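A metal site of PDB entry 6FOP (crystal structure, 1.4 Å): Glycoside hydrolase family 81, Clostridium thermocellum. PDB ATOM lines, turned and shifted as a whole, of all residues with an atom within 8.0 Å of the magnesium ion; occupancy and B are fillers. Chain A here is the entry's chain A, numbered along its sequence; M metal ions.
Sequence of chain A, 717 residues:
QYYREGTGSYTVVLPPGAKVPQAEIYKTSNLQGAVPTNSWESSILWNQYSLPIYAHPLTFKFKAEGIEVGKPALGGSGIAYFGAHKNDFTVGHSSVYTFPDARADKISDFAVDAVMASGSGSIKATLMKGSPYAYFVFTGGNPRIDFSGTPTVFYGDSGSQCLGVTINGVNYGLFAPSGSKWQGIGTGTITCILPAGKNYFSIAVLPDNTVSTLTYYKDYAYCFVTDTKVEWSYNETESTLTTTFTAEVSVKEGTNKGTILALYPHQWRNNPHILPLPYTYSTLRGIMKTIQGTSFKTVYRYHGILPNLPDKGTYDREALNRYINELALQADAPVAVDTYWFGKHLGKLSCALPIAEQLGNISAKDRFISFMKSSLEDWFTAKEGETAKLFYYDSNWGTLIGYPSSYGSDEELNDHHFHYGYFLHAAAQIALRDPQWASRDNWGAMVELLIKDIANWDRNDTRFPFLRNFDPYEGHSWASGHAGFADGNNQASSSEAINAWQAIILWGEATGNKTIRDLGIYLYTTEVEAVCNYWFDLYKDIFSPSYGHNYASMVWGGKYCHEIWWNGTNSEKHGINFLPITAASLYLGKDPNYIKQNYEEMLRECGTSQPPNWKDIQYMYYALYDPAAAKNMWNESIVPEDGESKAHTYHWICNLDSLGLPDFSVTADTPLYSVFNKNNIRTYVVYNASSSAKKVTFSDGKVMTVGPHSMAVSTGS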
ATOM      1  N   ILE A  25       9.972  32.845 -19.223  1.00  0.00           N
ATOM      2  CA  ILE A  25       9.018  31.740 -19.167  1.00  0.00           C
ATOM      3  C   ILE A  25       8.619  31.382 -20.591  1.00  0.00           C
ATOM      4  O   ILE A  25       8.035  32.203 -21.308  1.00  0.00           O
ATOM      5  CB  ILE A  25       7.777  32.060 -18.325  1.00  0.00           C
ATOM      6  CG1 ILE A  25       8.179  32.537 -16.925  1.00  0.00           C
ATOM      7  CG2 ILE A  25       6.907  30.798 -18.182  1.00  0.00           C
ATOM      8  CD1 ILE A  25       7.030  32.843 -15.991  1.00  0.00           C
ATOM      9  N   TYR A  26       8.943  30.162 -21.003  1.00  0.00           N
ATOM     10  CA  TYR A  26       8.696  29.692 -22.361  1.00  0.00           C
ATOM     11  C   TYR A  26       7.237  29.213 -22.444  1.00  0.00           C
ATOM     12  O   TYR A  26       6.910  28.018 -22.416  1.00  0.00           O
ATOM     13  CB  TYR A  26       9.742  28.635 -22.799  1.00  0.00           C
ATOM     14  CG  TYR A  26      11.086  29.241 -23.032  1.00  0.00           C
ATOM     15  CD1 TYR A  26      11.404  29.818 -24.269  1.00  0.00           C
ATOM     16  CD2 TYR A  26      12.070  29.267 -22.019  1.00  0.00           C
ATOM     17  CE1 TYR A  26      12.642  30.412 -24.483  1.00  0.00           C
ATOM     18  CE2 TYR A  26      13.309  29.848 -22.232  1.00  0.00           C
ATOM     19  CZ  TYR A  26      13.599  30.409 -23.469  1.00  0.00           C
ATOM     20  OH  TYR A  26      14.817  30.981 -23.703  1.00  0.00           O
ATOM     21  N   LYS A  27       6.362  30.208 -22.542  1.00  0.00           N
ATOM     22  CA  LYS A  27       4.927  30.032 -22.666  1.00  0.00           C
ATOM     23  C   LYS A  27       4.438  30.920 -23.815  1.00  0.00           C
ATOM     24  O   LYS A  27       5.096  31.911 -24.181  1.00  0.00           O
ATOM     25  CB  LYS A  27       4.183  30.368 -21.357  1.00  0.00           C
ATOM     26  CG  LYS A  27       4.338  31.801 -20.875  1.00  0.00           C
ATOM     27  CD  LYS A  27       3.513  32.033 -19.614  1.00  0.00           C
ATOM     28  CE  LYS A  27       3.934  33.294 -18.892  1.00  0.00           C
ATOM     29  NZ  LYS A  27       3.575  34.505 -19.661  1.00  0.00           N
ATOM     30  N   GLU A  41       5.766  17.982 -17.053  1.00  0.00           N
ATOM     31  CA  GLU A  41       5.868  18.800 -18.261  1.00  0.00           C
ATOM     32  C   GLU A  41       6.705  20.073 -18.044  1.00  0.00           C
ATOM     33  O   GLU A  41       6.940  20.843 -18.969  1.00  0.00           O
ATOM     34  CB  GLU A  41       4.487  19.164 -18.793  1.00  0.00           C
ATOM     35  CG  GLU A  41       3.773  20.302 -18.043  1.00  0.00           C
ATOM     36  CD  GLU A  41       3.252  19.984 -16.668  1.00  0.00           C
ATOM     37  OE1 GLU A  41       3.084  18.799 -16.338  1.00  0.00           O
ATOM     38  OE2 GLU A  41       2.906  20.973 -15.947  1.00  0.00           O
ATOM     39  N   SER A  42       7.147  20.320 -16.806  1.00  0.00           N
ATOM     40  CA  SER A  42       7.633  21.635 -16.416  1.00  0.00           C
ATOM     41  C   SER A  42       8.825  22.152 -17.168  1.00  0.00           C
ATOM     42  O   SER A  42       8.968  23.364 -17.309  1.00  0.00           O
ATOM     43  CB  SER A  42       7.890  21.664 -14.912  1.00  0.00           C
ATOM     44  OG  SER A  42       6.703  21.401 -14.209  1.00  0.00           O
ATOM     45  N   SER A  43       9.709  21.258 -17.624  1.00  0.00           N
ATOM     46  CA  SER A  43      10.943  21.751 -18.285  1.00  0.00           C
ATOM     47  C   SER A  43      10.695  22.508 -19.596  1.00  0.00           C
ATOM     48  O   SER A  43      11.530  23.320 -20.004  1.00  0.00           O
ATOM     49  CB  SER A  43      11.934  20.613 -18.541  1.00  0.00           C
ATOM     50  OG  SER A  43      11.521  19.785 -19.628  1.00  0.00           O
ATOM     51  N   ILE A  44       9.536  22.298 -20.196  1.00  0.00           N
ATOM     52  CA  ILE A  44       9.114  23.111 -21.341  1.00  0.00           C
ATOM     53  C   ILE A  44       9.120  24.595 -21.033  1.00  0.00           C
ATOM     54  O   ILE A  44       9.544  25.396 -21.877  1.00  0.00           O
ATOM     55  CB  ILE A  44       7.736  22.696 -21.866  1.00  0.00           C
ATOM     56  CG1 ILE A  44       7.709  21.228 -22.294  1.00  0.00           C
ATOM     57  CG2 ILE A  44       7.304  23.572 -23.024  1.00  0.00           C
ATOM     58  CD1 ILE A  44       6.319  20.670 -22.474  1.00  0.00           C
ATOM     59  N   LEU A  45       8.687  24.954 -19.821  1.00  0.00           N
ATOM     60  CA  LEU A  45       8.576  26.346 -19.392  1.00  0.00           C
ATOM     61  C   LEU A  45       9.911  26.985 -19.066  1.00  0.00           C
ATOM     62  O   LEU A  45      10.084  28.196 -19.266  1.00  0.00           O
ATOM     63  CB  LEU A  45       7.664  26.453 -18.157  1.00  0.00           C
ATOM     64  CG  LEU A  45       6.187  26.136 -18.417  1.00  0.00           C
ATOM     65  CD1 LEU A  45       5.517  25.681 -17.129  1.00  0.00           C
ATOM     66  CD2 LEU A  45       5.467  27.317 -19.039  1.00  0.00           C
ATOM     67  N   TRP A  46      10.843  26.193 -18.504  1.00  0.00           N
ATOM     68  CA  TRP A  46      12.088  26.744 -17.976  1.00  0.00           C
ATOM     69  C   TRP A  46      13.240  26.747 -18.991  1.00  0.00           C
ATOM     70  O   TRP A  46      14.153  27.580 -18.908  1.00  0.00           O
ATOM     71  CB  TRP A  46      12.508  25.935 -16.731  1.00  0.00           C
ATOM     72  CG  TRP A  46      11.611  26.056 -15.517  1.00  0.00           C
ATOM     73  CD1 TRP A  46      10.424  25.413 -15.310  1.00  0.00           C
ATOM     74  CD2 TRP A  46      11.885  26.782 -14.328  1.00  0.00           C
ATOM     75  NE1 TRP A  46       9.922  25.714 -14.057  1.00  0.00           N
ATOM     76  CE2 TRP A  46      10.814  26.566 -13.434  1.00  0.00           C
ATOM     77  CE3 TRP A  46      12.944  27.597 -13.922  1.00  0.00           C
ATOM     78  CZ2 TRP A  46      10.783  27.114 -12.153  1.00  0.00           C
ATOM     79  CZ3 TRP A  46      12.898  28.158 -12.661  1.00  0.00           C
ATOM     80  CH2 TRP A  46      11.836  27.905 -11.796  1.00  0.00           C
ATOM     81  N   ASN A  47      13.227  25.772 -19.897  1.00  0.00           N
ATOM     82  CA  ASN A  47      14.280  25.580 -20.877  1.00  0.00           C
ATOM     83  C   ASN A  47      13.809  26.107 -22.243  1.00  0.00           C
ATOM     84  O   ASN A  47      12.631  26.099 -22.539  1.00  0.00           O
ATOM     85  CB  ASN A  47      14.590  24.070 -20.889  1.00  0.00           C
ATOM     86  CG  ASN A  47      15.851  23.719 -21.619  1.00  0.00           C
ATOM     87  OD1 ASN A  47      16.975  23.770 -21.085  1.00  0.00           O
ATOM     88  ND2 ASN A  47      15.671  23.314 -22.838  1.00  0.00           N
ATOM     89  N   GLN A  48      14.763  26.569 -23.067  1.00  0.00           N
ATOM     90  CA  GLN A  48      14.436  27.003 -24.427  1.00  0.00           C
ATOM     91  C   GLN A  48      13.561  25.944 -25.123  1.00  0.00           C
ATOM     92  O   GLN A  48      12.522  26.249 -25.698  1.00  0.00           O
ATOM     93  CB  GLN A  48      15.738  27.240 -25.188  1.00  0.00           C
ATOM     94  CG  GLN A  48      15.576  27.656 -26.626  1.00  0.00           C
ATOM     95  CD  GLN A  48      16.904  27.940 -27.309  1.00  0.00           C
ATOM     96  OE1 GLN A  48      17.966  27.748 -26.737  1.00  0.00           O
ATOM     97  NE2 GLN A  48      16.838  28.367 -28.546  1.00  0.00           N
ATOM     98  N   TYR A  49      14.050  24.703 -25.112  1.00  0.00           N
ATOM     99  CA  TYR A  49      13.331  23.585 -25.672  1.00  0.00           C
ATOM    100  C   TYR A  49      12.662  22.814 -24.514  1.00  0.00           C
ATOM    101  O   TYR A  49      11.687  23.304 -23.974  1.00  0.00           O
ATOM    102  CB  TYR A  49      14.275  22.762 -26.581  1.00  0.00           C
ATOM    103  CG  TYR A  49      14.739  23.558 -27.784  1.00  0.00           C
ATOM    104  CD1 TYR A  49      13.861  23.883 -28.808  1.00  0.00           C
ATOM    105  CD2 TYR A  49      16.035  24.061 -27.853  1.00  0.00           C
ATOM    106  CE1 TYR A  49      14.275  24.646 -29.890  1.00  0.00           C
ATOM    107  CE2 TYR A  49      16.458  24.790 -28.934  1.00  0.00           C
ATOM    108  CZ  TYR A  49      15.580  25.101 -29.938  1.00  0.00           C
ATOM    109  OH  TYR A  49      16.015  25.874 -30.990  1.00  0.00           O
ATOM    110  N   SER A  50      13.193  21.652 -24.135  1.00  0.00           N
ATOM    111  CA  SER A  50      12.802  20.979 -22.925  1.00  0.00           C
ATOM    112  C   SER A  50      13.891  20.009 -22.546  1.00  0.00           C
ATOM    113  O   SER A  50      14.824  19.757 -23.334  1.00  0.00           O
ATOM    114  CB  SER A  50      11.491  20.183 -23.096  1.00  0.00           C
ATOM    115  OG  SER A  50      11.671  18.941 -23.779  1.00  0.00           O
ATOM    116  N   LEU A  51      13.744  19.423 -21.366  1.00  0.00           N
ATOM    117  CA  LEU A  51      14.441  18.190 -20.992  1.00  0.00           C
ATOM    118  C   LEU A  51      13.465  17.042 -21.295  1.00  0.00           C
ATOM    119  O   LEU A  51      12.336  17.284 -21.760  1.00  0.00           O
ATOM    120  CB  LEU A  51      14.861  18.204 -19.506  1.00  0.00           C
ATOM    121  CG  LEU A  51      16.188  18.905 -19.212  1.00  0.00           C
ATOM    122  CD1 LEU A  51      17.373  18.125 -19.768  1.00  0.00           C
ATOM    123  CD2 LEU A  51      16.233  20.350 -19.653  1.00  0.00           C
ATOM    124  N   PHE A  62      11.742  18.049 -26.599  1.00  0.00           N
ATOM    125  CA  PHE A  62      11.768  19.118 -27.617  1.00  0.00           C
ATOM    126  C   PHE A  62      13.215  19.477 -27.910  1.00  0.00           C
ATOM    127  O   PHE A  62      14.061  19.451 -27.027  1.00  0.00           O
ATOM    128  CB  PHE A  62      10.990  20.351 -27.121  1.00  0.00           C
ATOM    129  CG  PHE A  62       9.505  20.104 -27.013  1.00  0.00           C
ATOM    130  CD1 PHE A  62       8.962  19.543 -25.860  1.00  0.00           C
ATOM    131  CD2 PHE A  62       8.648  20.435 -28.067  1.00  0.00           C
ATOM    132  CE1 PHE A  62       7.612  19.293 -25.770  1.00  0.00           C
ATOM    133  CE2 PHE A  62       7.292  20.178 -27.977  1.00  0.00           C
ATOM    134  CZ  PHE A  62       6.776  19.618 -26.814  1.00  0.00           C
ATOM    135  N   PRO A 100      12.881  28.025 -33.032  1.00  0.00           N
ATOM    136  CA  PRO A 100      13.665  28.806 -32.068  1.00  0.00           C
ATOM    137  C   PRO A 100      13.480  28.384 -30.614  1.00  0.00           C
ATOM    138  O   PRO A 100      14.366  28.633 -29.800  1.00  0.00           O
ATOM    139  CB  PRO A 100      13.121  30.229 -32.256  1.00  0.00           C
ATOM    140  CG  PRO A 100      11.754  30.050 -32.749  1.00  0.00           C
ATOM    141  CD  PRO A 100      11.787  28.816 -33.615  1.00  0.00           C
ATOM    142  N   ASP A 101      12.378  27.721 -30.296  1.00  0.00           N
ATOM    143  CA  ASP A 101      12.066  27.305 -28.914  1.00  0.00           C
ATOM    144  C   ASP A 101      10.851  26.399 -28.919  1.00  0.00           C
ATOM    145  O   ASP A 101      10.250  26.180 -29.980  1.00  0.00           O
ATOM    146  CB  ASP A 101      11.857  28.512 -27.989  1.00  0.00           C
ATOM    147  CG  ASP A 101      10.741  29.450 -28.428  1.00  0.00           C
ATOM    148  OD1 ASP A 101       9.675  29.009 -28.868  1.00  0.00           O
ATOM    149  OD2 ASP A 101      10.916  30.681 -28.260  1.00  0.00           O
ATOM    150  N   ALA A 102      10.482  25.881 -27.745  1.00  0.00           N
ATOM    151  CA  ALA A 102       9.212  25.207 -27.529  1.00  0.00           C
ATOM    152  C   ALA A 102       8.574  25.890 -26.331  1.00  0.00           C
ATOM    153  O   ALA A 102       9.235  26.040 -25.276  1.00  0.00           O
ATOM    154  CB  ALA A 102       9.410  23.738 -27.263  1.00  0.00           C
ATOM    155  N   ARG A 103       7.295  26.251 -26.491  1.00  0.00           N
ATOM    156  CA  ARG A 103       6.558  27.008 -25.478  1.00  0.00           C
ATOM    157  C   ARG A 103       5.279  26.306 -25.070  1.00  0.00           C
ATOM    158  O   ARG A 103       4.553  25.786 -25.903  1.00  0.00           O
ATOM    159  CB  ARG A 103       6.210  28.392 -25.982  1.00  0.00           C
ATOM    160  CG  ARG A 103       7.437  29.270 -26.186  1.00  0.00           C
ATOM    161  CD  ARG A 103       7.136  30.594 -26.848  1.00  0.00           C
ATOM    162  NE  ARG A 103       8.356  31.414 -26.880  1.00  0.00           N
ATOM    163  CZ  ARG A 103       8.674  32.365 -25.989  1.00  0.00           C
ATOM    164  NH1 ARG A 103       7.884  32.682 -24.960  1.00  0.00           N
ATOM    165  NH2 ARG A 103       9.832  33.009 -26.126  1.00  0.00           N
ATOM    166  N   ALA A 104       4.972  26.319 -23.764  1.00  0.00           N
ATOM    167  CA  ALA A 104       3.701  25.747 -23.301  1.00  0.00           C
ATOM    168  C   ALA A 104       2.556  26.700 -23.651  1.00  0.00           C
ATOM    169  O   ALA A 104       2.625  27.882 -23.372  1.00  0.00           O
ATOM    170  CB  ALA A 104       3.722  25.490 -21.801  1.00  0.00           C
ATOM    171  N   ALA A 114       2.061  22.128 -26.388  1.00  0.00           N
ATOM    172  CA  ALA A 114       3.232  22.988 -26.612  1.00  0.00           C
ATOM    173  C   ALA A 114       3.342  23.357 -28.085  1.00  0.00           C
ATOM    174  O   ALA A 114       2.953  22.567 -28.943  1.00  0.00           O
ATOM    175  CB  ALA A 114       4.508  22.284 -26.159  1.00  0.00           C
ATOM    176  N   VAL A 115       3.884  24.538 -28.339  1.00  0.00           N
ATOM    177  CA  VAL A 115       3.993  25.060 -29.697  1.00  0.00           C
ATOM    178  C   VAL A 115       5.450  25.356 -30.008  1.00  0.00           C
ATOM    179  O   VAL A 115       6.173  25.946 -29.188  1.00  0.00           O
ATOM    180  CB  VAL A 115       3.184  26.375 -29.845  1.00  0.00           C
ATOM    181  CG1 VAL A 115       3.437  27.023 -31.216  1.00  0.00           C
ATOM    182  CG2 VAL A 115       1.713  26.117 -29.656  1.00  0.00           C
HETATM  183 MG    MG M   1      10.823  25.506 -23.794  1.00  0.00          MG
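Tyr 26 touches the magnesium ion (CB to MG, 3.5 Å).
The backbone NH (N) of Ala 102 is in hydrogen-bond range of the backbone carbonyl oxygen (O) of Gln 48, at 2.9 Å.
ND2 of Asn 47 lies close to N of Tyr 49.
The backbone NH (N) of Ser 50 lies close to the side-chain amide nitrogen (ND2) of Asn 47, at 3.3 Å.
OH of Tyr 49 lies within hydrogen-bond range of O of Pro 100.
O of Pro 100 is in hydrogen-bond range of NE2 of Gln 48, at 2.8 Å.
The backbone NH of Tyr 26 is in hydrogen-bond range of the backbone carbonyl oxygen of Leu 45 (2.9 Å).
N of Ala 104 sits at hydrogen-bond distance from O of Tyr 26 (2.9 Å).
The magnesium ion is bound by the backbone carbonyl oxygen of Ala 102 (2.2 Å), the backbone carbonyl oxygen of Asn 47 (2.3 Å), the backbone carbonyl oxygen of Ile 44 (2.3 Å) and the backbone carbonyl oxygen of Tyr 49 (2.4 Å).
Slightly farther from the magnesium ion lies O of Gln 48 (2.7 Å).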
